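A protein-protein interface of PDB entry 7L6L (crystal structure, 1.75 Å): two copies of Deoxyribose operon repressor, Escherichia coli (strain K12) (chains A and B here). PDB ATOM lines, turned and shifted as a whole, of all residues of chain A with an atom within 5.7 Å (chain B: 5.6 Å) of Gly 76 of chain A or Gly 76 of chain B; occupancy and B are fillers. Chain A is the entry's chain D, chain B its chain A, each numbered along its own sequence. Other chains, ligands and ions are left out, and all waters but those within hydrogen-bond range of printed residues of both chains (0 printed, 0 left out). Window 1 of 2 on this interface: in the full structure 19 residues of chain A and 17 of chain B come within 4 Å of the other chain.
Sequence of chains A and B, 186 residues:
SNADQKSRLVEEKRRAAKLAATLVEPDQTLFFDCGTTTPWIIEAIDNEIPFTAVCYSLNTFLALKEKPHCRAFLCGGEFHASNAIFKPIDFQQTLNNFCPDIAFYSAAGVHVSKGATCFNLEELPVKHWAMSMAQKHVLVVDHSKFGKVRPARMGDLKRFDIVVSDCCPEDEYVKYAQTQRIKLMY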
ATOM      1  N   LEU A  74      -5.955 -17.412  22.793  1.00  0.00           N
ATOM      2  CA  LEU A  74      -4.708 -17.776  23.507  1.00  0.00           C
ATOM      3  C   LEU A  74      -4.474 -16.751  24.617  1.00  0.00           C
ATOM      4  O   LEU A  74      -4.560 -15.537  24.324  1.00  0.00           O
ATOM      5  CB  LEU A  74      -3.532 -17.798  22.523  1.00  0.00           C
ATOM      6  CG  LEU A  74      -2.146 -18.063  23.121  1.00  0.00           C
ATOM      7  CD1 LEU A  74      -2.101 -19.378  23.886  1.00  0.00           C
ATOM      8  CD2 LEU A  74      -1.093 -18.074  22.021  1.00  0.00           C
ATOM      9  N   CYS A  75      -4.275 -17.238  25.842  1.00  0.00           N
ATOM     10  CA  CYS A  75      -3.888 -16.411  27.015  1.00  0.00           C
ATOM     11  C   CYS A  75      -2.411 -16.066  26.810  1.00  0.00           C
ATOM     12  O   CYS A  75      -1.608 -17.007  26.691  1.00  0.00           O
ATOM     13  CB  CYS A  75      -4.110 -17.179  28.314  1.00  0.00           C
ATOM     14  SG  CYS A  75      -3.416 -16.384  29.791  1.00  0.00           S
ATOM     15  N   GLY A  76      -2.080 -14.781  26.720  1.00  0.00           N
ATOM     16  CA  GLY A  76      -0.691 -14.367  26.461  1.00  0.00           C
ATOM     17  C   GLY A  76       0.113 -14.189  27.735  1.00  0.00           C
ATOM     18  O   GLY A  76      -0.372 -14.548  28.818  1.00  0.00           O
ATOM     19  N   GLY A  77       1.317 -13.651  27.601  1.00  0.00           N
ATOM     20  CA  GLY A  77       2.228 -13.420  28.732  1.00  0.00           C
ATOM     21  C   GLY A  77       3.642 -13.853  28.401  1.00  0.00           C
ATOM     22  O   GLY A  77       3.992 -13.924  27.198  1.00  0.00           O
ATOM     23  N   GLU A  78       4.412 -14.175  29.439  1.00  0.00           N
ATOM     24  CA  GLU A  78       5.826 -14.576  29.247  1.00  0.00           C
ATOM     25  C   GLU A  78       5.878 -16.048  28.837  1.00  0.00           C
ATOM     26  O   GLU A  78       5.199 -16.876  29.491  1.00  0.00           O
ATOM     27  CB  GLU A  78       6.619 -14.346  30.530  1.00  0.00           C
ATOM     28  CG  GLU A  78       8.102 -14.593  30.342  1.00  0.00           C
ATOM     29  CD  GLU A  78       8.969 -14.238  31.532  1.00  0.00           C
ATOM     30  OE1 GLU A  78       8.449 -13.646  32.502  1.00  0.00           O
ATOM     31  OE2 GLU A  78      10.170 -14.540  31.478  1.00  0.00           O
ATOM     32  N   PHE A  86       2.382 -19.815  28.404  1.00  0.00           N
ATOM     33  CA  PHE A  86       2.416 -18.339  28.492  1.00  0.00           C
ATOM     34  C   PHE A  86       1.895 -17.992  29.886  1.00  0.00           C
ATOM     35  O   PHE A  86       0.770 -18.416  30.225  1.00  0.00           O
ATOM     36  CB  PHE A  86       1.608 -17.693  27.367  1.00  0.00           C
ATOM     37  CG  PHE A  86       2.185 -17.959  26.005  1.00  0.00           C
ATOM     38  CD1 PHE A  86       3.212 -17.169  25.507  1.00  0.00           C
ATOM     39  CD2 PHE A  86       1.734 -19.022  25.240  1.00  0.00           C
ATOM     40  CE1 PHE A  86       3.753 -17.426  24.260  1.00  0.00           C
ATOM     41  CE2 PHE A  86       2.278 -19.274  23.990  1.00  0.00           C
ATOM     42  CZ  PHE A  86       3.288 -18.478  23.507  1.00  0.00           C
ATOM     43  N   LYS A  87       2.706 -17.283  30.671  1.00  0.00           N
ATOM     44  CA  LYS A  87       2.319 -16.892  32.051  1.00  0.00           C
ATOM     45  C   LYS A  87       2.040 -15.392  32.087  1.00  0.00           C
ATOM     46  O   LYS A  87       2.938 -14.586  31.841  1.00  0.00           O
ATOM     47  CB  LYS A  87       3.435 -17.247  33.037  1.00  0.00           C
ATOM     48  CG  LYS A  87       3.099 -17.012  34.503  1.00  0.00           C
ATOM     49  CD  LYS A  87       4.264 -17.270  35.431  1.00  0.00           C
ATOM     50  CE  LYS A  87       3.886 -17.216  36.895  1.00  0.00           C
ATOM     51  NZ  LYS A  87       3.332 -15.898  37.284  1.00  0.00           N
ATOM     52  N   PRO A  88       0.792 -14.968  32.371  1.00  0.00           N
ATOM     53  CA  PRO A  88       0.481 -13.545  32.453  1.00  0.00           C
ATOM     54  C   PRO A  88       1.329 -12.864  33.538  1.00  0.00           C
ATOM     55  O   PRO A  88       1.599 -13.481  34.560  1.00  0.00           O
ATOM     56  CB  PRO A  88      -1.009 -13.522  32.832  1.00  0.00           C
ATOM     57  CG  PRO A  88      -1.531 -14.854  32.343  1.00  0.00           C
ATOM     58  CD  PRO A  88      -0.392 -15.818  32.590  1.00  0.00           C
ATOM     59  N   THR A  94      -7.158 -11.615  29.164  1.00  0.00           N
ATOM     60  CA  THR A  94      -7.910 -12.492  28.228  1.00  0.00           C
ATOM     61  C   THR A  94      -8.835 -13.421  29.020  1.00  0.00           C
ATOM     62  O   THR A  94     -10.039 -13.398  28.752  1.00  0.00           O
ATOM     63  CB  THR A  94      -6.990 -13.302  27.304  1.00  0.00           C
ATOM     64  OG1 THR A  94      -6.252 -12.392  26.488  1.00  0.00           O
ATOM     65  CG2 THR A  94      -7.759 -14.251  26.408  1.00  0.00           C
ATOM     66  N   LEU B  74       4.085 -12.874  24.421  1.00  0.00           N
ATOM     67  CA  LEU B  74       3.076 -12.878  23.331  1.00  0.00           C
ATOM     68  C   LEU B  74       1.816 -12.181  23.844  1.00  0.00           C
ATOM     69  O   LEU B  74       1.379 -12.489  24.976  1.00  0.00           O
ATOM     70  CB  LEU B  74       2.794 -14.318  22.884  1.00  0.00           C
ATOM     71  CG  LEU B  74       1.748 -14.504  21.779  1.00  0.00           C
ATOM     72  CD1 LEU B  74       2.106 -13.738  20.517  1.00  0.00           C
ATOM     73  CD2 LEU B  74       1.578 -15.979  21.442  1.00  0.00           C
ATOM     74  N   CYS B  75       1.341 -11.195  23.087  1.00  0.00           N
ATOM     75  CA  CYS B  75       0.049 -10.519  23.363  1.00  0.00           C
ATOM     76  C   CYS B  75      -1.032 -11.502  22.916  1.00  0.00           C
ATOM     77  O   CYS B  75      -1.032 -11.859  21.719  1.00  0.00           O
ATOM     78  CB  CYS B  75      -0.037  -9.192  22.615  1.00  0.00           C
ATOM     79  SG  CYS B  75      -1.643  -8.356  22.734  1.00  0.00           S
ATOM     80  N   GLY B  76      -1.870 -11.960  23.845  1.00  0.00           N
ATOM     81  CA  GLY B  76      -2.906 -12.954  23.518  1.00  0.00           C
ATOM     82  C   GLY B  76      -4.182 -12.326  22.990  1.00  0.00           C
ATOM     83  O   GLY B  76      -4.207 -11.106  22.730  1.00  0.00           O
ATOM     84  N   GLY B  77      -5.222 -13.139  22.854  1.00  0.00           N
ATOM     85  CA  GLY B  77      -6.516 -12.654  22.353  1.00  0.00           C
ATOM     86  C   GLY B  77      -7.104 -13.660  21.386  1.00  0.00           C
ATOM     87  O   GLY B  77      -6.694 -14.829  21.445  1.00  0.00           O
ATOM     88  N   GLU B  78      -8.030 -13.214  20.541  1.00  0.00           N
ATOM     89  CA  GLU B  78      -8.667 -14.113  19.550  1.00  0.00           C
ATOM     90  C   GLU B  78      -7.713 -14.295  18.368  1.00  0.00           C
ATOM     91  O   GLU B  78      -7.193 -13.287  17.871  1.00  0.00           O
ATOM     92  CB  GLU B  78      -9.991 -13.513  19.079  1.00  0.00           C
ATOM     93  CG  GLU B  78     -10.748 -14.421  18.140  1.00  0.00           C
ATOM     94  CD  GLU B  78     -12.135 -13.932  17.767  1.00  0.00           C
ATOM     95  OE1 GLU B  78     -12.563 -12.890  18.304  1.00  0.00           O
ATOM     96  OE2 GLU B  78     -12.790 -14.614  16.963  1.00  0.00           O
ATOM     97  N   PHE B  86      -3.129 -12.349  17.025  1.00  0.00           N
ATOM     98  CA  PHE B  86      -3.989 -12.454  18.222  1.00  0.00           C
ATOM     99  C   PHE B  86      -4.520 -11.046  18.471  1.00  0.00           C
ATOM    100  O   PHE B  86      -3.703 -10.108  18.572  1.00  0.00           O
ATOM    101  CB  PHE B  86      -3.223 -13.037  19.411  1.00  0.00           C
ATOM    102  CG  PHE B  86      -2.739 -14.441  19.162  1.00  0.00           C
ATOM    103  CD1 PHE B  86      -3.585 -15.523  19.359  1.00  0.00           C
ATOM    104  CD2 PHE B  86      -1.465 -14.679  18.682  1.00  0.00           C
ATOM    105  CE1 PHE B  86      -3.148 -16.817  19.112  1.00  0.00           C
ATOM    106  CE2 PHE B  86      -1.035 -15.973  18.424  1.00  0.00           C
ATOM    107  CZ  PHE B  86      -1.873 -17.039  18.650  1.00  0.00           C
ATOM    108  N   LYS B  87      -5.841 -10.898  18.508  1.00  0.00           N
ATOM    109  CA  LYS B  87      -6.462  -9.567  18.742  1.00  0.00           C
ATOM    110  C   LYS B  87      -7.059  -9.539  20.147  1.00  0.00           C
ATOM    111  O   LYS B  87      -7.967 -10.309  20.454  1.00  0.00           O
ATOM    112  CB  LYS B  87      -7.536  -9.273  17.691  1.00  0.00           C
ATOM    113  CG  LYS B  87      -8.225  -7.924  17.842  1.00  0.00           C
ATOM    114  CD  LYS B  87      -9.367  -7.710  16.871  1.00  0.00           C
ATOM    115  CE  LYS B  87     -10.145  -6.445  17.158  1.00  0.00           C
ATOM    116  NZ  LYS B  87     -11.360  -6.335  16.317  1.00  0.00           N
ATOM    117  N   PRO B  88      -6.556  -8.667  21.051  1.00  0.00           N
ATOM    118  CA  PRO B  88      -7.108  -8.579  22.397  1.00  0.00           C
ATOM    119  C   PRO B  88      -8.603  -8.248  22.335  1.00  0.00           C
ATOM    120  O   PRO B  88      -9.018  -7.509  21.442  1.00  0.00           O
ATOM    121  CB  PRO B  88      -6.338  -7.422  23.050  1.00  0.00           C
ATOM    122  CG  PRO B  88      -5.041  -7.358  22.272  1.00  0.00           C
ATOM    123  CD  PRO B  88      -5.416  -7.753  20.858  1.00  0.00           C
ATOM    124  N   THR B  94      -1.231  -7.231  28.811  1.00  0.00           N
ATOM    125  CA  THR B  94       0.179  -7.647  28.576  1.00  0.00           C
ATOM    126  C   THR B  94       0.976  -6.473  28.003  1.00  0.00           C
ATOM    127  O   THR B  94       2.037  -6.175  28.552  1.00  0.00           O
ATOM    128  CB  THR B  94       0.274  -8.867  27.650  1.00  0.00           C
ATOM    129  OG1 THR B  94      -0.320  -9.992  28.298  1.00  0.00           O
ATOM    130  CG2 THR B  94       1.696  -9.240  27.292  1.00  0.00           C
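Printed residues of chain B that touch a printed residue of chain A: Leu 74, Gly 76, Gly 77 and Phe 86. Hydrophobic or aromatic side chains of chain B that line the printed part of chain A: Leu 74 and Phe 86. Hydrophobic or aromatic side chains of chain A that line the printed part of chain B: Leu 74 and Phe 86.
Among the printed residues, pairs that only touch across the chains: Gly 76 of chain A with Leu 74 of chain B, Leu 74 of chain A with Gly 76 of chain B, Leu 74 of chain A with Leu 74 of chain B, Phe 86 of chain A with Leu 74 of chain B, Leu 74 of chain A with Phe 86 of chain B, Gly 76 of chain A with Gly 76 of chain B and Thr 94 of chain A with Gly 77 of chain B.
The backbone NH (N) of Gly 77 of chain B lies within hydrogen-bond range of the backbone carbonyl oxygen (O) of Leu 74 of chain A. N of Gly 77 of chain A is in hydrogen-bond range of O of Leu 74 of chain B (2.9 Å).
Gly 76 of chain A touches just these residues of chain B: Leu 74 and Gly 76. Printed residues of chain B within 4 Å of Phe 86 of chain A: Leu 74. Lys 87 of chain A touches none of the printed residues of chain B. Printed residues of chain B within 4 Å of Thr 94 of chain A: Gly 77. Of the printed residues of chain A, Leu 74 of chain B touches Leu 74, Gly 76, Gly 77 and Phe 86. Of the printed residues of chain A, Gly 76 of chain B touches Leu 74 and Gly 76. Printed residues of chain A within 4 Å of Phe 86 of chain B: Leu 74. The nearest residue of chain B that does not touch Gly 76 of chain A is Thr 94 of chain B (4.3 Å).
Leu 74 of chain B touches its own counterpart, Leu 74 of chain A. Leu 74 of chain A touches Gly 77 of chain B, and with the chains exchanged Gly 77 of chain A touches Leu 74 of chain B. Leu 74 of chain A touches Phe 86 of chain B, and with the chains exchanged Phe 86 of chain A touches Leu 74 of chain B. Gly 76 of chain B touches its own counterpart, Gly 76 of chain A. 9 positions are printed for both chains. Of the 9 pairs that touch across the chains among the printed residues, 8 have their exchanged pair printed and touching as well.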
